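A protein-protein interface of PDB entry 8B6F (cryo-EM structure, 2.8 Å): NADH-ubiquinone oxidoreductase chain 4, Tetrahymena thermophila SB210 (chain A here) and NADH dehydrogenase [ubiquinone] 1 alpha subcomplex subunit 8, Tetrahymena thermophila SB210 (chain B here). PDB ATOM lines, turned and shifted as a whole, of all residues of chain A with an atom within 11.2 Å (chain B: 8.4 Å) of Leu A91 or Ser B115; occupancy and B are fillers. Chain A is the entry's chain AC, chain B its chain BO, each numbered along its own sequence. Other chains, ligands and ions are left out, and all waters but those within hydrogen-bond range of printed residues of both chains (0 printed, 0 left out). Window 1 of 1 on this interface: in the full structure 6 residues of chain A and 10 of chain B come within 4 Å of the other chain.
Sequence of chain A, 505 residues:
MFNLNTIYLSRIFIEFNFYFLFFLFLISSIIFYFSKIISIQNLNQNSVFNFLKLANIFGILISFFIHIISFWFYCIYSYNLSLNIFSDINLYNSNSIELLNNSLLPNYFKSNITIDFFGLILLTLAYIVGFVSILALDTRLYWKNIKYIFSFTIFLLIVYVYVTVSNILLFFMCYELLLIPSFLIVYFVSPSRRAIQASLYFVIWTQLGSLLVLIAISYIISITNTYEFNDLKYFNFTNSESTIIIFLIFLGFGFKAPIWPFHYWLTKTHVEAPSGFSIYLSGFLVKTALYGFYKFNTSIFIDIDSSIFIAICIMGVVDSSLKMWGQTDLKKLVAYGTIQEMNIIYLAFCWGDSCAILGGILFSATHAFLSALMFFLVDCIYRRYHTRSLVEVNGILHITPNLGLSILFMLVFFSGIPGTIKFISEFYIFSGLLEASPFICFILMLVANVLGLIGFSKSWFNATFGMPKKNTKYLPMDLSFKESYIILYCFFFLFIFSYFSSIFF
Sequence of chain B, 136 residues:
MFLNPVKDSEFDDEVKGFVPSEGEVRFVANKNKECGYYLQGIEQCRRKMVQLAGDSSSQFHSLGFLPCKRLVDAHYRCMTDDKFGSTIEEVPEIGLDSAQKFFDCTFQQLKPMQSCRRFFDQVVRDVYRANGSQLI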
ATOM      1  N   ILE A  85      12.130   5.924  19.759  1.00  0.00           N
ATOM      2  CA  ILE A  85      10.916   6.672  19.460  1.00  0.00           C
ATOM      3  C   ILE A  85      10.151   6.017  18.315  1.00  0.00           C
ATOM      4  O   ILE A  85       8.925   5.868  18.372  1.00  0.00           O
ATOM      5  CB  ILE A  85      11.261   8.140  19.142  1.00  0.00           C
ATOM      6  CG1 ILE A  85      11.907   8.825  20.353  1.00  0.00           C
ATOM      7  CG2 ILE A  85      10.022   8.900  18.688  1.00  0.00           C
ATOM      8  CD1 ILE A  85      10.993   8.997  21.547  1.00  0.00           C
ATOM      9  N   PHE A  86      10.862   5.613  17.261  1.00  0.00           N
ATOM     10  CA  PHE A  86      10.214   5.154  16.038  1.00  0.00           C
ATOM     11  C   PHE A  86       9.672   3.736  16.166  1.00  0.00           C
ATOM     12  O   PHE A  86       8.619   3.420  15.601  1.00  0.00           O
ATOM     13  CB  PHE A  86      11.206   5.243  14.873  1.00  0.00           C
ATOM     14  CG  PHE A  86      10.839   4.395  13.688  1.00  0.00           C
ATOM     15  CD1 PHE A  86       9.962   4.872  12.729  1.00  0.00           C
ATOM     16  CD2 PHE A  86      11.391   3.136  13.517  1.00  0.00           C
ATOM     17  CE1 PHE A  86       9.628   4.103  11.631  1.00  0.00           C
ATOM     18  CE2 PHE A  86      11.060   2.361  12.421  1.00  0.00           C
ATOM     19  CZ  PHE A  86      10.178   2.846  11.476  1.00  0.00           C
ATOM     20  N   SER A  87      10.368   2.870  16.903  1.00  0.00           N
ATOM     21  CA  SER A  87      10.076   1.441  16.830  1.00  0.00           C
ATOM     22  C   SER A  87       8.699   1.119  17.396  1.00  0.00           C
ATOM     23  O   SER A  87       7.896   0.437  16.749  1.00  0.00           O
ATOM     24  CB  SER A  87      11.156   0.649  17.568  1.00  0.00           C
ATOM     25  OG  SER A  87      11.207   1.008  18.938  1.00  0.00           O
ATOM     26  N   ASP A  88       8.405   1.596  18.602  1.00  0.00           N
ATOM     27  CA  ASP A  88       7.193   1.179  19.294  1.00  0.00           C
ATOM     28  C   ASP A  88       5.966   1.845  18.684  1.00  0.00           C
ATOM     29  O   ASP A  88       5.955   3.057  18.450  1.00  0.00           O
ATOM     30  CB  ASP A  88       7.294   1.513  20.780  1.00  0.00           C
ATOM     31  CG  ASP A  88       6.281   0.757  21.614  1.00  0.00           C
ATOM     32  OD1 ASP A  88       5.439   0.049  21.025  1.00  0.00           O
ATOM     33  OD2 ASP A  88       6.332   0.864  22.856  1.00  0.00           O
ATOM     34  N   ILE A  89       4.929   1.048  18.433  1.00  0.00           N
ATOM     35  CA  ILE A  89       3.687   1.545  17.848  1.00  0.00           C
ATOM     36  C   ILE A  89       2.490   1.379  18.771  1.00  0.00           C
ATOM     37  O   ILE A  89       1.425   1.944  18.479  1.00  0.00           O
ATOM     38  CB  ILE A  89       3.392   0.871  16.491  1.00  0.00           C
ATOM     39  CG1 ILE A  89       3.401  -0.653  16.646  1.00  0.00           C
ATOM     40  CG2 ILE A  89       4.404   1.329  15.450  1.00  0.00           C
ATOM     41  CD1 ILE A  89       3.014  -1.408  15.393  1.00  0.00           C
ATOM     42  N   ASN A  90       2.613   0.628  19.863  1.00  0.00           N
ATOM     43  CA  ASN A  90       1.496   0.465  20.782  1.00  0.00           C
ATOM     44  C   ASN A  90       1.121   1.806  21.400  1.00  0.00           C
ATOM     45  O   ASN A  90       1.987   2.590  21.797  1.00  0.00           O
ATOM     46  CB  ASN A  90       1.855  -0.541  21.875  1.00  0.00           C
ATOM     47  CG  ASN A  90       0.687  -0.849  22.789  1.00  0.00           C
ATOM     48  OD1 ASN A  90      -0.457  -0.510  22.489  1.00  0.00           O
ATOM     49  ND2 ASN A  90       0.968  -1.504  23.908  1.00  0.00           N
ATOM     50  N   LEU A  91      -0.186   2.068  21.482  1.00  0.00           N
ATOM     51  CA  LEU A  91      -0.650   3.365  21.962  1.00  0.00           C
ATOM     52  C   LEU A  91      -0.435   3.526  23.460  1.00  0.00           C
ATOM     53  O   LEU A  91      -0.225   4.647  23.935  1.00  0.00           O
ATOM     54  CB  LEU A  91      -2.125   3.556  21.617  1.00  0.00           C
ATOM     55  CG  LEU A  91      -2.486   3.456  20.132  1.00  0.00           C
ATOM     56  CD1 LEU A  91      -3.972   3.702  19.925  1.00  0.00           C
ATOM     57  CD2 LEU A  91      -1.666   4.428  19.298  1.00  0.00           C
ATOM     58  N   TYR A  92      -0.498   2.433  24.221  1.00  0.00           N
ATOM     59  CA  TYR A  92      -0.291   2.531  25.661  1.00  0.00           C
ATOM     60  C   TYR A  92       1.162   2.851  25.991  1.00  0.00           C
ATOM     61  O   TYR A  92       1.441   3.574  26.954  1.00  0.00           O
ATOM     62  CB  TYR A  92      -0.722   1.235  26.346  1.00  0.00           C
ATOM     63  CG  TYR A  92      -2.217   1.019  26.364  1.00  0.00           C
ATOM     64  CD1 TYR A  92      -2.858   0.364  25.321  1.00  0.00           C
ATOM     65  CD2 TYR A  92      -2.986   1.466  27.430  1.00  0.00           C
ATOM     66  CE1 TYR A  92      -4.225   0.164  25.337  1.00  0.00           C
ATOM     67  CE2 TYR A  92      -4.353   1.272  27.455  1.00  0.00           C
ATOM     68  CZ  TYR A  92      -4.967   0.620  26.407  1.00  0.00           C
ATOM     69  OH  TYR A  92      -6.327   0.426  26.431  1.00  0.00           O
ATOM     70  N   ASN A  93       2.098   2.326  25.208  1.00  0.00           N
ATOM     71  CA  ASN A  93       3.514   2.509  25.493  1.00  0.00           C
ATOM     72  C   ASN A  93       4.017   3.833  24.932  1.00  0.00           C
ATOM     73  O   ASN A  93       3.633   4.248  23.836  1.00  0.00           O
ATOM     74  CB  ASN A  93       4.325   1.357  24.900  1.00  0.00           C
ATOM     75  CG  ASN A  93       3.936   0.014  25.481  1.00  0.00           C
ATOM     76  OD1 ASN A  93       3.460  -0.073  26.611  1.00  0.00           O
ATOM     77  ND2 ASN A  93       4.137  -1.044  24.705  1.00  0.00           N
ATOM     78  N   SER A  94       4.881   4.493  25.698  1.00  0.00           N
ATOM     79  CA  SER A  94       5.502   5.741  25.279  1.00  0.00           C
ATOM     80  C   SER A  94       6.883   5.830  25.911  1.00  0.00           C
ATOM     81  O   SER A  94       7.072   5.411  27.056  1.00  0.00           O
ATOM     82  CB  SER A  94       4.648   6.950  25.679  1.00  0.00           C
ATOM     83  OG  SER A  94       5.258   8.163  25.283  1.00  0.00           O
ATOM     84  N   ASN A  95       7.842   6.377  25.167  1.00  0.00           N
ATOM     85  CA  ASN A  95       9.224   6.477  25.636  1.00  0.00           C
ATOM     86  C   ASN A  95       9.354   7.717  26.511  1.00  0.00           C
ATOM     87  O   ASN A  95       9.505   8.833  26.012  1.00  0.00           O
ATOM     88  CB  ASN A  95      10.198   6.527  24.465  1.00  0.00           C
ATOM     89  CG  ASN A  95      11.632   6.719  24.911  1.00  0.00           C
ATOM     90  OD1 ASN A  95      11.971   6.490  26.070  1.00  0.00           O
ATOM     91  ND2 ASN A  95      12.486   7.144  23.986  1.00  0.00           N
ATOM     92  N   SER A  96       9.297   7.521  27.827  1.00  0.00           N
ATOM     93  CA  SER A  96       9.461   8.596  28.805  1.00  0.00           C
ATOM     94  C   SER A  96      10.501   8.129  29.818  1.00  0.00           C
ATOM     95  O   SER A  96      10.158   7.562  30.858  1.00  0.00           O
ATOM     96  CB  SER A  96       8.136   8.945  29.471  1.00  0.00           C
ATOM     97  OG  SER A  96       7.209   9.452  28.528  1.00  0.00           O
ATOM     98  N   ILE A  97      11.771   8.374  29.507  1.00  0.00           N
ATOM     99  CA  ILE A  97      12.889   8.035  30.379  1.00  0.00           C
ATOM    100  C   ILE A  97      13.512   9.336  30.863  1.00  0.00           C
ATOM    101  O   ILE A  97      13.851  10.209  30.056  1.00  0.00           O
ATOM    102  CB  ILE A  97      13.919   7.149  29.657  1.00  0.00           C
ATOM    103  CG1 ILE A  97      15.001   6.694  30.640  1.00  0.00           C
ATOM    104  CG2 ILE A  97      14.537   7.884  28.468  1.00  0.00           C
ATOM    105  CD1 ILE A  97      16.017   5.734  30.047  1.00  0.00           C
ATOM    106  N   MET B   1      -2.207   4.107  15.499  1.00  0.00           N
ATOM    107  CA  MET B   1      -2.926   5.412  15.446  1.00  0.00           C
ATOM    108  C   MET B   1      -3.250   5.764  13.998  1.00  0.00           C
ATOM    109  O   MET B   1      -2.371   5.746  13.137  1.00  0.00           O
ATOM    110  CB  MET B   1      -2.084   6.514  16.092  1.00  0.00           C
ATOM    111  CG  MET B   1      -2.892   7.702  16.595  1.00  0.00           C
ATOM    112  SD  MET B   1      -1.869   8.923  17.444  1.00  0.00           S
ATOM    113  CE  MET B   1      -3.106  10.097  17.989  1.00  0.00           C
ATOM    114  N   PHE B   2      -4.518   6.079  13.736  1.00  0.00           N
ATOM    115  CA  PHE B   2      -4.998   6.362  12.384  1.00  0.00           C
ATOM    116  C   PHE B   2      -4.885   5.138  11.483  1.00  0.00           C
ATOM    117  O   PHE B   2      -4.750   5.262  10.264  1.00  0.00           O
ATOM    118  CB  PHE B   2      -4.247   7.547  11.765  1.00  0.00           C
ATOM    119  CG  PHE B   2      -4.225   8.768  12.634  1.00  0.00           C
ATOM    120  CD1 PHE B   2      -5.376   9.511  12.834  1.00  0.00           C
ATOM    121  CD2 PHE B   2      -3.052   9.178  13.244  1.00  0.00           C
ATOM    122  CE1 PHE B   2      -5.357  10.637  13.631  1.00  0.00           C
ATOM    123  CE2 PHE B   2      -3.029  10.303  14.043  1.00  0.00           C
ATOM    124  CZ  PHE B   2      -4.183  11.033  14.237  1.00  0.00           C
ATOM    125  N   LEU B   3      -4.936   3.949  12.077  1.00  0.00           N
ATOM    126  CA  LEU B   3      -4.887   2.688  11.349  1.00  0.00           C
ATOM    127  C   LEU B   3      -6.167   1.909  11.610  1.00  0.00           C
ATOM    128  O   LEU B   3      -6.588   1.769  12.763  1.00  0.00           O
ATOM    129  CB  LEU B   3      -3.669   1.858  11.765  1.00  0.00           C
ATOM    130  CG  LEU B   3      -2.408   2.028  10.915  1.00  0.00           C
ATOM    131  CD1 LEU B   3      -1.998   3.483  10.820  1.00  0.00           C
ATOM    132  CD2 LEU B   3      -1.275   1.205  11.489  1.00  0.00           C
ATOM    133  N   ARG B  46      -3.238  14.250  39.209  1.00  0.00           N
ATOM    134  CA  ARG B  46      -3.015  12.820  39.397  1.00  0.00           C
ATOM    135  C   ARG B  46      -1.820  12.575  40.308  1.00  0.00           C
ATOM    136  O   ARG B  46      -1.897  11.783  41.254  1.00  0.00           O
ATOM    137  CB  ARG B  46      -2.816  12.141  38.041  1.00  0.00           C
ATOM    138  CG  ARG B  46      -2.618  10.635  38.131  1.00  0.00           C
ATOM    139  CD  ARG B  46      -2.435  10.007  36.762  1.00  0.00           C
ATOM    140  NE  ARG B  46      -1.214  10.460  36.107  1.00  0.00           N
ATOM    141  CZ  ARG B  46      -0.721   9.937  34.993  1.00  0.00           C
ATOM    142  NH1 ARG B  46      -1.318   8.929  34.380  1.00  0.00           N
ATOM    143  NH2 ARG B  46       0.400  10.436  34.483  1.00  0.00           N
ATOM    144  N   LYS B 101     -10.822   3.194  27.436  1.00  0.00           N
ATOM    145  CA  LYS B 101      -9.393   2.997  27.220  1.00  0.00           C
ATOM    146  C   LYS B 101      -8.585   4.133  27.833  1.00  0.00           C
ATOM    147  O   LYS B 101      -7.531   3.900  28.435  1.00  0.00           O
ATOM    148  CB  LYS B 101      -9.098   2.878  25.726  1.00  0.00           C
ATOM    149  CG  LYS B 101      -9.604   1.592  25.093  1.00  0.00           C
ATOM    150  CD  LYS B 101      -9.225   1.517  23.621  1.00  0.00           C
ATOM    151  CE  LYS B 101      -9.664   0.203  22.997  1.00  0.00           C
ATOM    152  NZ  LYS B 101     -11.141   0.022  23.053  1.00  0.00           N
ATOM    153  N   PHE B 102      -9.055   5.373  27.682  1.00  0.00           N
ATOM    154  CA  PHE B 102      -8.350   6.503  28.276  1.00  0.00           C
ATOM    155  C   PHE B 102      -8.314   6.403  29.794  1.00  0.00           C
ATOM    156  O   PHE B 102      -7.277   6.661  30.416  1.00  0.00           O
ATOM    157  CB  PHE B 102      -9.007   7.818  27.856  1.00  0.00           C
ATOM    158  CG  PHE B 102      -8.716   8.958  28.788  1.00  0.00           C
ATOM    159  CD1 PHE B 102      -7.528   9.662  28.689  1.00  0.00           C
ATOM    160  CD2 PHE B 102      -9.629   9.326  29.761  1.00  0.00           C
ATOM    161  CE1 PHE B 102      -7.254  10.712  29.545  1.00  0.00           C
ATOM    162  CE2 PHE B 102      -9.362  10.374  30.621  1.00  0.00           C
ATOM    163  CZ  PHE B 102      -8.172  11.069  30.510  1.00  0.00           C
ATOM    164  N   CYS B 105      -5.825   3.871  30.777  1.00  0.00           N
ATOM    165  CA  CYS B 105      -4.479   4.403  30.588  1.00  0.00           C
ATOM    166  C   CYS B 105      -4.079   5.319  31.736  1.00  0.00           C
ATOM    167  O   CYS B 105      -2.951   5.243  32.236  1.00  0.00           O
ATOM    168  CB  CYS B 105      -4.401   5.161  29.262  1.00  0.00           C
ATOM    169  SG  CYS B 105      -2.812   5.979  28.931  1.00  0.00           S
ATOM    170  N   THR B 106      -4.987   6.191  32.169  1.00  0.00           N
ATOM    171  CA  THR B 106      -4.609   7.255  33.091  1.00  0.00           C
ATOM    172  C   THR B 106      -4.593   6.777  34.538  1.00  0.00           C
ATOM    173  O   THR B 106      -3.617   7.006  35.259  1.00  0.00           O
ATOM    174  CB  THR B 106      -5.566   8.440  32.936  1.00  0.00           C
ATOM    175  OG1 THR B 106      -5.614   8.842  31.563  1.00  0.00           O
ATOM    176  CG2 THR B 106      -5.108   9.622  33.779  1.00  0.00           C
ATOM    177  N   GLN B 109      -3.526   1.888  34.762  1.00  0.00           N
ATOM    178  CA  GLN B 109      -2.157   1.595  34.361  1.00  0.00           C
ATOM    179  C   GLN B 109      -1.194   2.720  34.710  1.00  0.00           C
ATOM    180  O   GLN B 109       0.021   2.495  34.712  1.00  0.00           O
ATOM    181  CB  GLN B 109      -2.103   1.314  32.859  1.00  0.00           C
ATOM    182  CG  GLN B 109      -2.994   0.160  32.428  1.00  0.00           C
ATOM    183  CD  GLN B 109      -2.875  -0.147  30.952  1.00  0.00           C
ATOM    184  OE1 GLN B 109      -1.941   0.298  30.287  1.00  0.00           O
ATOM    185  NE2 GLN B 109      -3.826  -0.911  30.428  1.00  0.00           N
ATOM    186  N   LEU B 110      -1.703   3.914  35.009  1.00  0.00           N
ATOM    187  CA  LEU B 110      -0.860   5.055  35.356  1.00  0.00           C
ATOM    188  C   LEU B 110       0.206   5.291  34.290  1.00  0.00           C
ATOM    189  O   LEU B 110       1.365   5.582  34.588  1.00  0.00           O
ATOM    190  CB  LEU B 110      -0.225   4.861  36.732  1.00  0.00           C
ATOM    191  CG  LEU B 110      -1.208   4.760  37.904  1.00  0.00           C
ATOM    192  CD1 LEU B 110      -0.481   4.472  39.197  1.00  0.00           C
ATOM    193  CD2 LEU B 110      -2.020   6.035  38.046  1.00  0.00           C
ATOM    194  N   LYS B 111      -0.194   5.160  33.033  1.00  0.00           N
ATOM    195  CA  LYS B 111       0.708   5.366  31.916  1.00  0.00           C
ATOM    196  C   LYS B 111       0.947   6.855  31.680  1.00  0.00           C
ATOM    197  O   LYS B 111       0.206   7.703  32.180  1.00  0.00           O
ATOM    198  CB  LYS B 111       0.136   4.720  30.658  1.00  0.00           C
ATOM    199  CG  LYS B 111       0.216   3.199  30.640  1.00  0.00           C
ATOM    200  CD  LYS B 111       1.649   2.714  30.473  1.00  0.00           C
ATOM    201  CE  LYS B 111       1.708   1.199  30.363  1.00  0.00           C
ATOM    202  NZ  LYS B 111       3.097   0.717  30.135  1.00  0.00           N
ATOM    203  N   PRO B 112       1.988   7.197  30.923  1.00  0.00           N
ATOM    204  CA  PRO B 112       2.294   8.612  30.680  1.00  0.00           C
ATOM    205  C   PRO B 112       1.151   9.326  29.976  1.00  0.00           C
ATOM    206  O   PRO B 112       0.403   8.738  29.191  1.00  0.00           O
ATOM    207  CB  PRO B 112       3.543   8.559  29.794  1.00  0.00           C
ATOM    208  CG  PRO B 112       4.169   7.255  30.102  1.00  0.00           C
ATOM    209  CD  PRO B 112       3.034   6.313  30.378  1.00  0.00           C
ATOM    210  N   MET B 113       1.029  10.624  30.264  1.00  0.00           N
ATOM    211  CA  MET B 113       0.025  11.443  29.594  1.00  0.00           C
ATOM    212  C   MET B 113       0.244  11.476  28.091  1.00  0.00           C
ATOM    213  O   MET B 113      -0.715  11.642  27.329  1.00  0.00           O
ATOM    214  CB  MET B 113       0.038  12.861  30.162  1.00  0.00           C
ATOM    215  CG  MET B 113      -0.289  12.929  31.642  1.00  0.00           C
ATOM    216  SD  MET B 113      -1.869  12.170  32.070  1.00  0.00           S
ATOM    217  CE  MET B 113      -3.003  13.125  31.065  1.00  0.00           C
ATOM    218  N   GLN B 114       1.491  11.327  27.640  1.00  0.00           N
ATOM    219  CA  GLN B 114       1.729  11.163  26.212  1.00  0.00           C
ATOM    220  C   GLN B 114       0.885  10.026  25.657  1.00  0.00           C
ATOM    221  O   GLN B 114       0.297  10.146  24.576  1.00  0.00           O
ATOM    222  CB  GLN B 114       3.213  10.900  25.941  1.00  0.00           C
ATOM    223  CG  GLN B 114       4.104  12.124  26.041  1.00  0.00           C
ATOM    224  CD  GLN B 114       4.372  12.540  27.469  1.00  0.00           C
ATOM    225  OE1 GLN B 114       3.836  11.956  28.409  1.00  0.00           O
ATOM    226  NE2 GLN B 114       5.214  13.551  27.641  1.00  0.00           N
ATOM    227  N   SER B 115       0.804   8.914  26.388  1.00  0.00           N
ATOM    228  CA  SER B 115       0.003   7.787  25.929  1.00  0.00           C
ATOM    229  C   SER B 115      -1.489   8.069  26.063  1.00  0.00           C
ATOM    230  O   SER B 115      -2.261   7.790  25.139  1.00  0.00           O
ATOM    231  CB  SER B 115       0.370   6.532  26.719  1.00  0.00           C
ATOM    232  OG  SER B 115       1.750   6.232  26.597  1.00  0.00           O
ATOM    233  N   CYS B 116      -1.919   8.619  27.199  1.00  0.00           N
ATOM    234  CA  CYS B 116      -3.351   8.730  27.460  1.00  0.00           C
ATOM    235  C   CYS B 116      -4.006   9.846  26.655  1.00  0.00           C
ATOM    236  O   CYS B 116      -5.205   9.765  26.368  1.00  0.00           O
ATOM    237  CB  CYS B 116      -3.603   8.940  28.953  1.00  0.00           C
ATOM    238  SG  CYS B 116      -2.815   7.703  30.016  1.00  0.00           S
ATOM    239  N   ARG B 117      -3.258  10.889  26.286  1.00  0.00           N
ATOM    240  CA  ARG B 117      -3.821  11.896  25.393  1.00  0.00           C
ATOM    241  C   ARG B 117      -4.225  11.289  24.060  1.00  0.00           C
ATOM    242  O   ARG B 117      -5.163  11.771  23.416  1.00  0.00           O
ATOM    243  CB  ARG B 117      -2.824  13.033  25.163  1.00  0.00           C
ATOM    244  CG  ARG B 117      -3.121  13.839  23.903  1.00  0.00           C
ATOM    245  CD  ARG B 117      -2.354  15.144  23.858  1.00  0.00           C
ATOM    246  NE  ARG B 117      -2.595  15.861  22.610  1.00  0.00           N
ATOM    247  CZ  ARG B 117      -2.198  17.102  22.366  1.00  0.00           C
ATOM    248  NH1 ARG B 117      -1.547  17.811  23.273  1.00  0.00           N
ATOM    249  NH2 ARG B 117      -2.456  17.644  21.179  1.00  0.00           N
ATOM    250  N   ARG B 118      -3.534  10.232  23.634  1.00  0.00           N
ATOM    251  CA  ARG B 118      -3.913   9.557  22.399  1.00  0.00           C
ATOM    252  C   ARG B 118      -5.337   9.032  22.488  1.00  0.00           C
ATOM    253  O   ARG B 118      -6.125   9.188  21.549  1.00  0.00           O
ATOM    254  CB  ARG B 118      -2.936   8.418  22.108  1.00  0.00           C
ATOM    255  CG  ARG B 118      -1.495   8.880  21.964  1.00  0.00           C
ATOM    256  CD  ARG B 118      -0.528   7.711  21.955  1.00  0.00           C
ATOM    257  NE  ARG B 118       0.854   8.165  22.032  1.00  0.00           N
ATOM    258  CZ  ARG B 118       1.902   7.365  22.160  1.00  0.00           C
ATOM    259  NH1 ARG B 118       1.767   6.051  22.226  1.00  0.00           N
ATOM    260  NH2 ARG B 118       3.119   7.897  22.228  1.00  0.00           N
ATOM    261  N   PHE B 119      -5.686   8.405  23.612  1.00  0.00           N
ATOM    262  CA  PHE B 119      -7.030   7.863  23.761  1.00  0.00           C
ATOM    263  C   PHE B 119      -8.063   8.968  23.941  1.00  0.00           C
ATOM    264  O   PHE B 119      -9.186   8.857  23.438  1.00  0.00           O
ATOM    265  CB  PHE B 119      -7.065   6.888  24.934  1.00  0.00           C
ATOM    266  CG  PHE B 119      -6.136   5.725  24.767  1.00  0.00           C
ATOM    267  CD1 PHE B 119      -6.453   4.693  23.902  1.00  0.00           C
ATOM    268  CD2 PHE B 119      -4.943   5.666  25.465  1.00  0.00           C
ATOM    269  CE1 PHE B 119      -5.601   3.622  23.738  1.00  0.00           C
ATOM    270  CE2 PHE B 119      -4.085   4.597  25.306  1.00  0.00           C
ATOM    271  CZ  PHE B 119      -4.416   3.572  24.442  1.00  0.00           C
ATOM    272  N   PHE B 120      -7.713  10.041  24.654  1.00  0.00           N
ATOM    273  CA  PHE B 120      -8.647  11.154  24.796  1.00  0.00           C
ATOM    274  C   PHE B 120      -8.932  11.794  23.443  1.00  0.00           C
ATOM    275  O   PHE B 120     -10.086  12.077  23.105  1.00  0.00           O
ATOM    276  CB  PHE B 120      -8.104  12.193  25.776  1.00  0.00           C
ATOM    277  CG  PHE B 120      -9.178  13.004  26.438  1.00  0.00           C
ATOM    278  CD1 PHE B 120      -9.769  14.065  25.774  1.00  0.00           C
ATOM    279  CD2 PHE B 120      -9.605  12.699  27.717  1.00  0.00           C
ATOM    280  CE1 PHE B 120     -10.764  14.809  26.378  1.00  0.00           C
ATOM    281  CE2 PHE B 120     -10.599  13.438  28.327  1.00  0.00           C
ATOM    282  CZ  PHE B 120     -11.179  14.494  27.656  1.00  0.00           C
ATOM    283  N   ASP B 121      -7.882  12.032  22.656  1.00  0.00           N
ATOM    284  CA  ASP B 121      -8.070  12.544  21.304  1.00  0.00           C
ATOM    285  C   ASP B 121      -8.850  11.565  20.444  1.00  0.00           C
ATOM    286  O   ASP B 121      -9.617  11.981  19.569  1.00  0.00           O
ATOM    287  CB  ASP B 121      -6.718  12.844  20.659  1.00  0.00           C
ATOM    288  CG  ASP B 121      -6.009  14.015  21.308  1.00  0.00           C
ATOM    289  OD1 ASP B 121      -6.560  14.585  22.273  1.00  0.00           O
ATOM    290  OD2 ASP B 121      -4.903  14.372  20.847  1.00  0.00           O
ATOM    291  N   GLN B 122      -8.689  10.265  20.688  1.00  0.00           N
ATOM    292  CA  GLN B 122      -9.483   9.283  19.961  1.00  0.00           C
ATOM    293  C   GLN B 122     -10.962   9.424  20.298  1.00  0.00           C
ATOM    294  O   GLN B 122     -11.819   9.299  19.417  1.00  0.00           O
ATOM    295  CB  GLN B 122      -8.987   7.871  20.270  1.00  0.00           C
ATOM    296  CG  GLN B 122      -9.750   6.771  19.545  1.00  0.00           C
ATOM    297  CD  GLN B 122      -9.751   6.955  18.038  1.00  0.00           C
ATOM    298  OE1 GLN B 122      -8.882   7.627  17.482  1.00  0.00           O
ATOM    299  NE2 GLN B 122     -10.728   6.356  17.368  1.00  0.00           N
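The backbone carbonyl oxygen (O) of Leu A91 sits at hydrogen-bond distance from the guanidinium group (NH1) of Arg B118 (3.0 Å).
O of Tyr A92 is in hydrogen-bond range of OG of Ser B115 (2.7 Å).
The backbone carbonyl oxygen (O) of Asn A90 lies within hydrogen-bond range of the guanidinium group (NH1) of Arg B118, 3.5 Å away.
O of Asn A93 sits at hydrogen-bond distance from NH1 of Arg B118, 3.1 Å away.
N of Lys B111 sits at hydrogen-bond distance from O of Cys B105, at 2.9 Å.
NH1 of Arg B46 is in hydrogen-bond range of O of Lys B111.
The backbone NH (N) of Asn A90 lies within hydrogen-bond range of the side-chain carboxylate (OD1) of Asp A88, at 3.1 Å.
The backbone carbonyl oxygen (O) of Gln B114 is in hydrogen-bond range of the guanidinium group (NE) of Arg B118 (3.3 Å).
OH of Tyr A92 touches CG of Lys B101 (3.7 Å).
CD2 of Tyr A92 touches OE1 of Gln B109, 3.3 Å away.
Lys B111 touches Tyr A92 (CD to O, 3.6 Å).
CZ of Phe B119 touches CE1 of Tyr A92, 3.5 Å away.
Asn A93 touches Lys B111.
OG of Ser B115 touches C of Asn A93 (3.7 Å).
OG of Ser A94 touches CB of Gln B114, 3.5 Å away.
Ser A94 touches Ser B115.
OG of Ser A94 touches NH2 of Arg B118 (3.7 Å).
Ser A96 touches Pro B112 (OG to CB, 3.98 Å).
Ser B115 touches just these residues of chain A: Leu A91 (3.4 Å), Tyr A92 (2.7 Å), Asn A93 (3.7 Å) and Ser A94 (3.1 Å).
Met B1 touches one residue of chain A.
Of chain A, only Ser A96 comes within 4 Å of Pro B112.
Of chain A, only Ser A94 comes within 4 Å of Gln B114.
Cys B116 touches none of the printed residues of chain A.
Arg B118 touches four residues of chain A.
Of the printed residues of chain B, Ser A96 touches Pro B112 (3.98 Å).
Printed residues of chain B within 4 Å of Tyr A92: Lys B101, Gln B109, Lys B111, Ser B115 and Phe B119.
Of the printed residues of chain B, Asn A90 touches Arg B118 (3.5 Å).
Asp A88 touches none of the printed residues of chain B.
Leu B110 touches none of the printed residues of chain A.
The nearest residue of chain B that does not touch Leu A91 is Cys B116 (5.4 Å).
The nearest residue of chain A that does not touch Ser B115 is Asn A90 (6.0 Å).
Printed residues of chain A that touch a printed residue of chain B: Asn A90, Leu A91, Tyr A92, Asn A93, Ser A94 and Ser A96.
Of the 22 printed residues of chain B, 9 touch a printed residue of chain A.
Among the printed residues, no Asp or Glu carboxylate lies within 4 Å of a Lys or Arg side-chain nitrogen of the other chain.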
